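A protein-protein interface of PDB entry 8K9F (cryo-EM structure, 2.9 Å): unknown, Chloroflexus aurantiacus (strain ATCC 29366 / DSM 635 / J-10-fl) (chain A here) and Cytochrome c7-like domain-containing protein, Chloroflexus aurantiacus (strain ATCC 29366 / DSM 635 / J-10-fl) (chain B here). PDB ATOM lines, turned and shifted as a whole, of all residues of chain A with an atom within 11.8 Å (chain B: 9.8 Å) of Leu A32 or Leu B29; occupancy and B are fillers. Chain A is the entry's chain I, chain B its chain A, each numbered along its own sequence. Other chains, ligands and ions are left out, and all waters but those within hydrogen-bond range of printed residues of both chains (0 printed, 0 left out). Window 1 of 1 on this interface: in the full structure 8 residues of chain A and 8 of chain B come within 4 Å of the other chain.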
ATOM      1  N   THR A  21      16.586   7.384  27.084  1.00  0.00           N
ATOM      2  CA  THR A  21      17.634   8.375  27.258  1.00  0.00           C
ATOM      3  C   THR A  21      17.987   9.107  25.982  1.00  0.00           C
ATOM      4  O   THR A  21      18.131  10.331  26.023  1.00  0.00           O
ATOM      5  CB  THR A  21      18.911   7.725  27.798  1.00  0.00           C
ATOM      6  OG1 THR A  21      18.587   6.678  28.719  1.00  0.00           O
ATOM      7  CG2 THR A  21      19.834   8.755  28.423  1.00  0.00           C
ATOM      8  N   GLY A  22      18.166   8.384  24.878  1.00  0.00           N
ATOM      9  CA  GLY A  22      18.514   8.989  23.611  1.00  0.00           C
ATOM     10  C   GLY A  22      17.438   9.916  23.088  1.00  0.00           C
ATOM     11  O   GLY A  22      17.725  11.067  22.752  1.00  0.00           O
ATOM     12  N   MET A  23      16.185   9.458  23.090  1.00  0.00           N
ATOM     13  CA  MET A  23      15.096  10.292  22.595  1.00  0.00           C
ATOM     14  C   MET A  23      14.694  11.388  23.572  1.00  0.00           C
ATOM     15  O   MET A  23      13.866  12.228  23.218  1.00  0.00           O
ATOM     16  CB  MET A  23      13.861   9.456  22.235  1.00  0.00           C
ATOM     17  CG  MET A  23      14.135   8.208  21.421  1.00  0.00           C
ATOM     18  SD  MET A  23      15.671   8.268  20.476  1.00  0.00           S
ATOM     19  CE  MET A  23      15.114   9.050  18.965  1.00  0.00           C
ATOM     20  N   VAL A  24      15.234  11.401  24.786  1.00  0.00           N
ATOM     21  CA  VAL A  24      15.016  12.557  25.648  1.00  0.00           C
ATOM     22  C   VAL A  24      16.158  13.553  25.496  1.00  0.00           C
ATOM     23  O   VAL A  24      15.931  14.729  25.191  1.00  0.00           O
ATOM     24  CB  VAL A  24      14.817  12.114  27.110  1.00  0.00           C
ATOM     25  CG1 VAL A  24      15.141  13.232  28.076  1.00  0.00           C
ATOM     26  CG2 VAL A  24      13.387  11.668  27.319  1.00  0.00           C
ATOM     27  N   ALA A  25      17.401  13.088  25.646  1.00  0.00           N
ATOM     28  CA  ALA A  25      18.553  13.980  25.633  1.00  0.00           C
ATOM     29  C   ALA A  25      18.823  14.557  24.249  1.00  0.00           C
ATOM     30  O   ALA A  25      19.005  15.773  24.117  1.00  0.00           O
ATOM     31  CB  ALA A  25      19.788  13.243  26.147  1.00  0.00           C
ATOM     32  N   PHE A  26      18.848  13.709  23.210  1.00  0.00           N
ATOM     33  CA  PHE A  26      19.122  14.188  21.861  1.00  0.00           C
ATOM     34  C   PHE A  26      18.008  15.098  21.357  1.00  0.00           C
ATOM     35  O   PHE A  26      18.279  16.102  20.690  1.00  0.00           O
ATOM     36  CB  PHE A  26      19.319  13.001  20.911  1.00  0.00           C
ATOM     37  CG  PHE A  26      19.061  13.328  19.468  1.00  0.00           C
ATOM     38  CD1 PHE A  26      19.979  14.075  18.743  1.00  0.00           C
ATOM     39  CD2 PHE A  26      17.901  12.895  18.835  1.00  0.00           C
ATOM     40  CE1 PHE A  26      19.746  14.388  17.418  1.00  0.00           C
ATOM     41  CE2 PHE A  26      17.659  13.210  17.514  1.00  0.00           C
ATOM     42  CZ  PHE A  26      18.586  13.955  16.804  1.00  0.00           C
ATOM     43  N   LEU A  27      16.750  14.772  21.673  1.00  0.00           N
ATOM     44  CA  LEU A  27      15.663  15.661  21.281  1.00  0.00           C
ATOM     45  C   LEU A  27      15.671  16.947  22.092  1.00  0.00           C
ATOM     46  O   LEU A  27      15.189  17.975  21.613  1.00  0.00           O
ATOM     47  CB  LEU A  27      14.309  14.962  21.407  1.00  0.00           C
ATOM     48  CG  LEU A  27      13.973  13.946  20.309  1.00  0.00           C
ATOM     49  CD1 LEU A  27      12.553  13.411  20.470  1.00  0.00           C
ATOM     50  CD2 LEU A  27      14.183  14.532  18.915  1.00  0.00           C
ATOM     51  N   LEU A  28      16.231  16.925  23.303  1.00  0.00           N
ATOM     52  CA  LEU A  28      16.397  18.165  24.051  1.00  0.00           C
ATOM     53  C   LEU A  28      17.449  19.064  23.412  1.00  0.00           C
ATOM     54  O   LEU A  28      17.262  20.285  23.340  1.00  0.00           O
ATOM     55  CB  LEU A  28      16.747  17.842  25.500  1.00  0.00           C
ATOM     56  CG  LEU A  28      15.530  17.834  26.424  1.00  0.00           C
ATOM     57  CD1 LEU A  28      15.966  17.597  27.838  1.00  0.00           C
ATOM     58  CD2 LEU A  28      14.769  19.141  26.331  1.00  0.00           C
ATOM     59  N   MET A  29      18.554  18.479  22.930  1.00  0.00           N
ATOM     60  CA  MET A  29      19.509  19.268  22.145  1.00  0.00           C
ATOM     61  C   MET A  29      18.908  19.728  20.824  1.00  0.00           C
ATOM     62  O   MET A  29      19.277  20.788  20.311  1.00  0.00           O
ATOM     63  CB  MET A  29      20.806  18.502  21.872  1.00  0.00           C
ATOM     64  CG  MET A  29      21.315  17.620  22.969  1.00  0.00           C
ATOM     65  SD  MET A  29      23.102  17.693  23.113  1.00  0.00           S
ATOM     66  CE  MET A  29      23.365  16.568  24.472  1.00  0.00           C
ATOM     67  N   VAL A  30      17.992  18.945  20.254  1.00  0.00           N
ATOM     68  CA  VAL A  30      17.309  19.367  19.034  1.00  0.00           C
ATOM     69  C   VAL A  30      16.401  20.562  19.314  1.00  0.00           C
ATOM     70  O   VAL A  30      16.373  21.530  18.543  1.00  0.00           O
ATOM     71  CB  VAL A  30      16.545  18.178  18.421  1.00  0.00           C
ATOM     72  CG1 VAL A  30      15.359  18.628  17.577  1.00  0.00           C
ATOM     73  CG2 VAL A  30      17.480  17.343  17.590  1.00  0.00           C
ATOM     74  N   TRP A  31      15.672  20.523  20.433  1.00  0.00           N
ATOM     75  CA  TRP A  31      14.767  21.613  20.788  1.00  0.00           C
ATOM     76  C   TRP A  31      15.560  22.872  21.116  1.00  0.00           C
ATOM     77  O   TRP A  31      15.204  23.963  20.659  1.00  0.00           O
ATOM     78  CB  TRP A  31      13.869  21.159  21.956  1.00  0.00           C
ATOM     79  CG  TRP A  31      12.886  22.140  22.658  1.00  0.00           C
ATOM     80  CD1 TRP A  31      12.773  23.499  22.510  1.00  0.00           C
ATOM     81  CD2 TRP A  31      11.886  21.773  23.624  1.00  0.00           C
ATOM     82  NE1 TRP A  31      11.777  23.991  23.317  1.00  0.00           N
ATOM     83  CE2 TRP A  31      11.215  22.951  24.009  1.00  0.00           C
ATOM     84  CE3 TRP A  31      11.493  20.557  24.196  1.00  0.00           C
ATOM     85  CZ2 TRP A  31      10.178  22.949  24.939  1.00  0.00           C
ATOM     86  CZ3 TRP A  31      10.464  20.559  25.117  1.00  0.00           C
ATOM     87  CH2 TRP A  31       9.819  21.746  25.482  1.00  0.00           C
ATOM     88  N   LEU A  32      16.656  22.737  21.871  1.00  0.00           N
ATOM     89  CA  LEU A  32      17.428  23.911  22.265  1.00  0.00           C
ATOM     90  C   LEU A  32      18.203  24.489  21.086  1.00  0.00           C
ATOM     91  O   LEU A  32      18.225  25.708  20.885  1.00  0.00           O
ATOM     92  CB  LEU A  32      18.383  23.553  23.405  1.00  0.00           C
ATOM     93  CG  LEU A  32      19.639  24.420  23.539  1.00  0.00           C
ATOM     94  CD1 LEU A  32      19.285  25.754  24.169  1.00  0.00           C
ATOM     95  CD2 LEU A  32      20.731  23.737  24.309  1.00  0.00           C
ATOM     96  N   PHE A  33      18.826  23.634  20.283  1.00  0.00           N
ATOM     97  CA  PHE A  33      19.749  24.087  19.259  1.00  0.00           C
ATOM     98  C   PHE A  33      19.092  24.387  17.922  1.00  0.00           C
ATOM     99  O   PHE A  33      19.772  24.886  17.021  1.00  0.00           O
ATOM    100  CB  PHE A  33      20.851  23.046  19.061  1.00  0.00           C
ATOM    101  CG  PHE A  33      21.829  22.967  20.200  1.00  0.00           C
ATOM    102  CD1 PHE A  33      22.340  24.123  20.769  1.00  0.00           C
ATOM    103  CD2 PHE A  33      22.255  21.744  20.688  1.00  0.00           C
ATOM    104  CE1 PHE A  33      23.254  24.059  21.806  1.00  0.00           C
ATOM    105  CE2 PHE A  33      23.157  21.671  21.727  1.00  0.00           C
ATOM    106  CZ  PHE A  33      23.659  22.831  22.289  1.00  0.00           C
ATOM    107  N   ALA A  34      17.803  24.100  17.755  1.00  0.00           N
ATOM    108  CA  ALA A  34      17.168  24.375  16.471  1.00  0.00           C
ATOM    109  C   ALA A  34      15.854  25.130  16.613  1.00  0.00           C
ATOM    110  O   ALA A  34      15.508  25.941  15.749  1.00  0.00           O
ATOM    111  CB  ALA A  34      16.941  23.077  15.698  1.00  0.00           C
ATOM    112  N   PHE A  35      15.104  24.862  17.682  1.00  0.00           N
ATOM    113  CA  PHE A  35      13.762  25.406  17.841  1.00  0.00           C
ATOM    114  C   PHE A  35      13.657  26.389  19.002  1.00  0.00           C
ATOM    115  O   PHE A  35      12.548  26.693  19.450  1.00  0.00           O
ATOM    116  CB  PHE A  35      12.740  24.283  18.033  1.00  0.00           C
ATOM    117  CG  PHE A  35      12.552  23.399  16.830  1.00  0.00           C
ATOM    118  CD1 PHE A  35      13.428  22.356  16.562  1.00  0.00           C
ATOM    119  CD2 PHE A  35      11.451  23.569  16.006  1.00  0.00           C
ATOM    120  CE1 PHE A  35      13.241  21.535  15.463  1.00  0.00           C
ATOM    121  CE2 PHE A  35      11.258  22.754  14.906  1.00  0.00           C
ATOM    122  CZ  PHE A  35      12.154  21.732  14.638  1.00  0.00           C
ATOM    123  N   TYR A  36      14.782  26.896  19.505  1.00  0.00           N
ATOM    124  CA  TYR A  36      14.785  27.739  20.702  1.00  0.00           C
ATOM    125  C   TYR A  36      15.590  28.991  20.361  1.00  0.00           C
ATOM    126  O   TYR A  36      16.775  29.088  20.688  1.00  0.00           O
ATOM    127  CB  TYR A  36      15.367  26.942  21.879  1.00  0.00           C
ATOM    128  CG  TYR A  36      15.250  27.489  23.283  1.00  0.00           C
ATOM    129  CD1 TYR A  36      15.864  28.671  23.674  1.00  0.00           C
ATOM    130  CD2 TYR A  36      14.588  26.748  24.252  1.00  0.00           C
ATOM    131  CE1 TYR A  36      15.761  29.129  24.964  1.00  0.00           C
ATOM    132  CE2 TYR A  36      14.475  27.198  25.538  1.00  0.00           C
ATOM    133  CZ  TYR A  36      15.064  28.383  25.888  1.00  0.00           C
ATOM    134  OH  TYR A  36      14.947  28.805  27.181  1.00  0.00           O
ATOM    135  N   TRP A  37      14.926  29.944  19.712  1.00  0.00           N
ATOM    136  CA  TRP A  37      15.491  31.249  19.367  1.00  0.00           C
ATOM    137  C   TRP A  37      14.367  32.187  18.950  1.00  0.00           C
ATOM    138  O   TRP A  37      14.609  33.328  18.563  1.00  0.00           O
ATOM    139  CB  TRP A  37      16.536  31.156  18.246  1.00  0.00           C
ATOM    140  CG  TRP A  37      16.179  30.264  17.091  1.00  0.00           C
ATOM    141  CD1 TRP A  37      16.343  28.912  17.017  1.00  0.00           C
ATOM    142  CD2 TRP A  37      15.635  30.671  15.830  1.00  0.00           C
ATOM    143  NE1 TRP A  37      15.918  28.450  15.796  1.00  0.00           N
ATOM    144  CE2 TRP A  37      15.478  29.509  15.049  1.00  0.00           C
ATOM    145  CE3 TRP A  37      15.256  31.906  15.288  1.00  0.00           C
ATOM    146  CZ2 TRP A  37      14.964  29.545  13.753  1.00  0.00           C
ATOM    147  CZ3 TRP A  37      14.744  31.937  14.001  1.00  0.00           C
ATOM    148  CH2 TRP A  37      14.601  30.765  13.250  1.00  0.00           C
ATOM    149  N   VAL B  21      27.283  10.700  31.989  1.00  0.00           N
ATOM    150  CA  VAL B  21      26.706  11.015  30.678  1.00  0.00           C
ATOM    151  C   VAL B  21      25.629  12.091  30.808  1.00  0.00           C
ATOM    152  O   VAL B  21      25.603  13.066  30.038  1.00  0.00           O
ATOM    153  CB  VAL B  21      26.163   9.736  30.012  1.00  0.00           C
ATOM    154  CG1 VAL B  21      25.221  10.065  28.865  1.00  0.00           C
ATOM    155  CG2 VAL B  21      27.306   8.876  29.509  1.00  0.00           C
ATOM    156  N   LEU B  22      24.772  11.970  31.828  1.00  0.00           N
ATOM    157  CA  LEU B  22      23.685  12.928  32.010  1.00  0.00           C
ATOM    158  C   LEU B  22      24.177  14.308  32.441  1.00  0.00           C
ATOM    159  O   LEU B  22      23.596  15.308  32.025  1.00  0.00           O
ATOM    160  CB  LEU B  22      22.668  12.389  33.014  1.00  0.00           C
ATOM    161  CG  LEU B  22      21.609  11.412  32.493  1.00  0.00           C
ATOM    162  CD1 LEU B  22      20.432  11.368  33.451  1.00  0.00           C
ATOM    163  CD2 LEU B  22      21.137  11.772  31.094  1.00  0.00           C
ATOM    164  N   LEU B  23      25.233  14.401  33.259  1.00  0.00           N
ATOM    165  CA  LEU B  23      25.761  15.725  33.594  1.00  0.00           C
ATOM    166  C   LEU B  23      26.526  16.351  32.440  1.00  0.00           C
ATOM    167  O   LEU B  23      26.564  17.578  32.344  1.00  0.00           O
ATOM    168  CB  LEU B  23      26.660  15.720  34.836  1.00  0.00           C
ATOM    169  CG  LEU B  23      26.345  15.072  36.181  1.00  0.00           C
ATOM    170  CD1 LEU B  23      27.605  15.009  37.038  1.00  0.00           C
ATOM    171  CD2 LEU B  23      25.231  15.820  36.901  1.00  0.00           C
ATOM    172  N   VAL B  24      27.140  15.549  31.563  1.00  0.00           N
ATOM    173  CA  VAL B  24      27.707  16.118  30.339  1.00  0.00           C
ATOM    174  C   VAL B  24      26.605  16.706  29.460  1.00  0.00           C
ATOM    175  O   VAL B  24      26.710  17.854  28.992  1.00  0.00           O
ATOM    176  CB  VAL B  24      28.533  15.052  29.593  1.00  0.00           C
ATOM    177  CG1 VAL B  24      28.807  15.475  28.157  1.00  0.00           C
ATOM    178  CG2 VAL B  24      29.843  14.802  30.320  1.00  0.00           C
ATOM    179  N   VAL B  25      25.515  15.950  29.275  1.00  0.00           N
ATOM    180  CA  VAL B  25      24.366  16.416  28.495  1.00  0.00           C
ATOM    181  C   VAL B  25      23.740  17.649  29.141  1.00  0.00           C
ATOM    182  O   VAL B  25      23.401  18.629  28.460  1.00  0.00           O
ATOM    183  CB  VAL B  25      23.348  15.267  28.338  1.00  0.00           C
ATOM    184  CG1 VAL B  25      22.006  15.766  27.828  1.00  0.00           C
ATOM    185  CG2 VAL B  25      23.899  14.189  27.412  1.00  0.00           C
ATOM    186  N   GLU B  26      23.649  17.650  30.471  1.00  0.00           N
ATOM    187  CA  GLU B  26      23.057  18.768  31.188  1.00  0.00           C
ATOM    188  C   GLU B  26      23.941  20.006  31.155  1.00  0.00           C
ATOM    189  O   GLU B  26      23.419  21.114  31.078  1.00  0.00           O
ATOM    190  CB  GLU B  26      22.768  18.371  32.634  1.00  0.00           C
ATOM    191  CG  GLU B  26      21.892  19.355  33.371  1.00  0.00           C
ATOM    192  CD  GLU B  26      20.563  19.575  32.675  1.00  0.00           C
ATOM    193  OE1 GLU B  26      19.662  18.730  32.848  1.00  0.00           O
ATOM    194  OE2 GLU B  26      20.408  20.597  31.972  1.00  0.00           O
ATOM    195  N   GLY B  27      25.264  19.849  31.220  1.00  0.00           N
ATOM    196  CA  GLY B  27      26.140  21.003  31.107  1.00  0.00           C
ATOM    197  C   GLY B  27      26.110  21.623  29.723  1.00  0.00           C
ATOM    198  O   GLY B  27      26.163  22.851  29.582  1.00  0.00           O
ATOM    199  N   ILE B  28      26.014  20.782  28.684  1.00  0.00           N
ATOM    200  CA  ILE B  28      25.798  21.291  27.329  1.00  0.00           C
ATOM    201  C   ILE B  28      24.467  22.036  27.244  1.00  0.00           C
ATOM    202  O   ILE B  28      24.375  23.108  26.626  1.00  0.00           O
ATOM    203  CB  ILE B  28      25.885  20.135  26.310  1.00  0.00           C
ATOM    204  CG1 ILE B  28      27.306  19.565  26.266  1.00  0.00           C
ATOM    205  CG2 ILE B  28      25.480  20.582  24.919  1.00  0.00           C
ATOM    206  CD1 ILE B  28      28.371  20.588  25.952  1.00  0.00           C
ATOM    207  N   LEU B  29      23.433  21.505  27.902  1.00  0.00           N
ATOM    208  CA  LEU B  29      22.130  22.165  27.938  1.00  0.00           C
ATOM    209  C   LEU B  29      22.189  23.493  28.694  1.00  0.00           C
ATOM    210  O   LEU B  29      21.553  24.467  28.283  1.00  0.00           O
ATOM    211  CB  LEU B  29      21.111  21.223  28.572  1.00  0.00           C
ATOM    212  CG  LEU B  29      20.106  20.549  27.645  1.00  0.00           C
ATOM    213  CD1 LEU B  29      19.147  19.744  28.447  1.00  0.00           C
ATOM    214  CD2 LEU B  29      19.341  21.572  26.876  1.00  0.00           C
ATOM    215  N   ILE B  30      22.970  23.544  29.779  1.00  0.00           N
ATOM    216  CA  ILE B  30      23.182  24.772  30.549  1.00  0.00           C
ATOM    217  C   ILE B  30      23.830  25.840  29.680  1.00  0.00           C
ATOM    218  O   ILE B  30      23.372  26.988  29.633  1.00  0.00           O
ATOM    219  CB  ILE B  30      24.049  24.480  31.793  1.00  0.00           C
ATOM    220  CG1 ILE B  30      23.285  23.757  32.906  1.00  0.00           C
ATOM    221  CG2 ILE B  30      24.662  25.756  32.361  1.00  0.00           C
ATOM    222  CD1 ILE B  30      21.859  24.111  33.036  1.00  0.00           C
ATOM    223  N   LEU B  31      24.903  25.464  28.971  1.00  0.00           N
ATOM    224  CA  LEU B  31      25.637  26.417  28.143  1.00  0.00           C
ATOM    225  C   LEU B  31      24.786  26.925  26.988  1.00  0.00           C
ATOM    226  O   LEU B  31      24.758  28.133  26.714  1.00  0.00           O
ATOM    227  CB  LEU B  31      26.917  25.774  27.614  1.00  0.00           C
ATOM    228  CG  LEU B  31      28.128  26.701  27.549  1.00  0.00           C
ATOM    229  CD1 LEU B  31      28.444  27.246  28.930  1.00  0.00           C
ATOM    230  CD2 LEU B  31      29.321  25.977  26.956  1.00  0.00           C
ATOM    231  N   GLY B  32      24.056  26.018  26.333  1.00  0.00           N
ATOM    232  CA  GLY B  32      23.194  26.422  25.239  1.00  0.00           C
ATOM    233  C   GLY B  32      22.042  27.302  25.680  1.00  0.00           C
ATOM    234  O   GLY B  32      21.713  28.287  25.009  1.00  0.00           O
ATOM    235  N   VAL B  33      21.414  26.958  26.810  1.00  0.00           N
ATOM    236  CA  VAL B  33      20.294  27.738  27.324  1.00  0.00           C
ATOM    237  C   VAL B  33      20.763  29.123  27.746  1.00  0.00           C
ATOM    238  O   VAL B  33      20.122  30.127  27.423  1.00  0.00           O
ATOM    239  CB  VAL B  33      19.603  26.983  28.477  1.00  0.00           C
ATOM    240  CG1 VAL B  33      18.876  27.934  29.423  1.00  0.00           C
ATOM    241  CG2 VAL B  33      18.629  25.964  27.925  1.00  0.00           C
ATOM    242  N   TYR B  34      21.914  29.202  28.428  1.00  0.00           N
ATOM    243  CA  TYR B  34      22.424  30.499  28.860  1.00  0.00           C
ATOM    244  C   TYR B  34      22.843  31.370  27.685  1.00  0.00           C
ATOM    245  O   TYR B  34      22.654  32.587  27.729  1.00  0.00           O
ATOM    246  CB  TYR B  34      23.603  30.337  29.816  1.00  0.00           C
ATOM    247  CG  TYR B  34      24.059  31.659  30.401  1.00  0.00           C
ATOM    248  CD1 TYR B  34      23.324  32.287  31.397  1.00  0.00           C
ATOM    249  CD2 TYR B  34      25.210  32.284  29.947  1.00  0.00           C
ATOM    250  CE1 TYR B  34      23.727  33.493  31.930  1.00  0.00           C
ATOM    251  CE2 TYR B  34      25.620  33.488  30.470  1.00  0.00           C
ATOM    252  CZ  TYR B  34      24.878  34.089  31.461  1.00  0.00           C
ATOM    253  OH  TYR B  34      25.290  35.292  31.986  1.00  0.00           O
ATOM    254  N   PHE B  35      23.410  30.784  26.631  1.00  0.00           N
ATOM    255  CA  PHE B  35      23.748  31.613  25.486  1.00  0.00           C
ATOM    256  C   PHE B  35      22.535  31.978  24.641  1.00  0.00           C
ATOM    257  O   PHE B  35      22.602  32.955  23.890  1.00  0.00           O
ATOM    258  CB  PHE B  35      24.806  30.927  24.632  1.00  0.00           C
ATOM    259  CG  PHE B  35      26.207  31.330  24.975  1.00  0.00           C
ATOM    260  CD1 PHE B  35      26.767  32.470  24.422  1.00  0.00           C
ATOM    261  CD2 PHE B  35      26.957  30.580  25.863  1.00  0.00           C
ATOM    262  CE1 PHE B  35      28.055  32.844  24.735  1.00  0.00           C
ATOM    263  CE2 PHE B  35      28.243  30.951  26.181  1.00  0.00           C
ATOM    264  CZ  PHE B  35      28.794  32.081  25.612  1.00  0.00           C
ATOM    265  N   ARG B  36      21.383  31.368  24.856  1.00  0.00           N
ATOM    266  CA  ARG B  36      20.208  31.781  24.111  1.00  0.00           C
ATOM    267  C   ARG B  36      19.206  32.403  25.037  1.00  0.00           C
ATOM    268  O   ARG B  36      18.112  32.753  24.627  1.00  0.00           O
ATOM    269  CB  ARG B  36      19.599  30.577  23.403  1.00  0.00           C
ATOM    270  CG  ARG B  36      20.296  30.229  22.109  1.00  0.00           C
ATOM    271  CD  ARG B  36      20.331  28.732  21.879  1.00  0.00           C
ATOM    272  NE  ARG B  36      21.406  28.363  20.970  1.00  0.00           N
ATOM    273  CZ  ARG B  36      22.674  28.237  21.342  1.00  0.00           C
ATOM    274  NH1 ARG B  36      23.010  28.461  22.598  1.00  0.00           N
ATOM    275  NH2 ARG B  36      23.603  27.900  20.464  1.00  0.00           N
ATOM    276  N   SER B  37      19.593  32.599  26.279  1.00  0.00           N
ATOM    277  CA  SER B  37      18.632  33.056  27.268  1.00  0.00           C
ATOM    278  C   SER B  37      18.195  34.490  27.000  1.00  0.00           C
ATOM    279  O   SER B  37      18.929  35.303  26.436  1.00  0.00           O
ATOM    280  CB  SER B  37      19.205  32.954  28.678  1.00  0.00           C
ATOM    281  OG  SER B  37      20.269  33.860  28.870  1.00  0.00           O
ATOM    282  N   TYR B 160      20.082  37.731  15.991  1.00  0.00           N
ATOM    283  CA  TYR B 160      21.009  36.660  15.650  1.00  0.00           C
ATOM    284  C   TYR B 160      21.388  36.708  14.172  1.00  0.00           C
ATOM    285  O   TYR B 160      20.779  37.420  13.378  1.00  0.00           O
ATOM    286  CB  TYR B 160      20.381  35.303  15.954  1.00  0.00           C
ATOM    287  CG  TYR B 160      20.258  34.948  17.411  1.00  0.00           C
ATOM    288  CD1 TYR B 160      21.280  35.221  18.300  1.00  0.00           C
ATOM    289  CD2 TYR B 160      19.106  34.349  17.903  1.00  0.00           C
ATOM    290  CE1 TYR B 160      21.171  34.888  19.632  1.00  0.00           C
ATOM    291  CE2 TYR B 160      18.986  34.017  19.233  1.00  0.00           C
ATOM    292  CZ  TYR B 160      20.027  34.286  20.091  1.00  0.00           C
ATOM    293  OH  TYR B 160      19.917  33.969  21.423  1.00  0.00           O
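The guanidinium group (NH1) of Arg B36 is in hydrogen-bond range of the backbone carbonyl oxygen (O) of Gly B32 (2.7 Å). O of Trp A31 is in hydrogen-bond range of N of Tyr A36 (3.2 Å). The backbone carbonyl oxygen (O) of Ala A34 lies within hydrogen-bond range of the indole nitrogen (NE1) of Trp A37 (2.5 Å).
Printed residues of chain B within 4 Å of Leu A32: Leu B29, Gly B32, Val B33 and Arg B36. Leu B29 touches just these residues of chain A: Leu A28 (3.9 Å) and Leu A32 (3.6 Å). Of the printed residues of chain A, Val B25 touches Ala A25 (3.8 Å) and Met A29 (3.7 Å). No residue of chain A comes within 4 Å of Glu B26. No residue of chain A comes within 4 Å of Gly B27. No residue of chain A comes within 4 Å of Ile B30. No residue of chain A comes within 4 Å of Leu B31. Printed residues of chain A within 4 Å of Tyr B160: Trp A37 (3.9 Å). Printed residues of chain B within 4 Å of Phe A33: Ile B28 and Arg B36. Of the printed residues of chain B, Tyr A36 touches Arg B36 (3.8 Å). Of the printed residues of chain B, Leu A28 touches Leu B29. Thr A21 touches none of the printed residues of chain B. The nearest residue of chain A that does not touch Leu B29 is Met A29 (5.1 Å). The nearest printed residue of chain B that does not touch Tyr A36 is Val B33 (4.6 Å).
Hydrophobic or aromatic side chains of chain B that line the printed part of chain A: Val B25, Ile B28, Leu B29, Val B33 and Tyr B160. Of the 17 printed residues of chain A, 7 touch a printed residue of chain B. Hydrophobic or aromatic side chains of chain A within 4 Å of the printed part of chain B: Ala A25, Leu A28, Met A29, Leu A32, Phe A33 and Trp A37. Among the printed residues, 11 pairs touch across the chains.
Among the printed residues, pairs that only touch across the chains: Leu A32 with Gly B32, Leu A32 with Val B33, Leu A32 with Leu B29, Met A29 with Val B25, Ala A25 with Val B25, Tyr A36 with Arg B36, Leu A32 with Arg B36, Leu A28 with Leu B29, Trp A37 with Tyr B160, Phe A33 with Ile B28 and Phe A33 with Arg B36.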
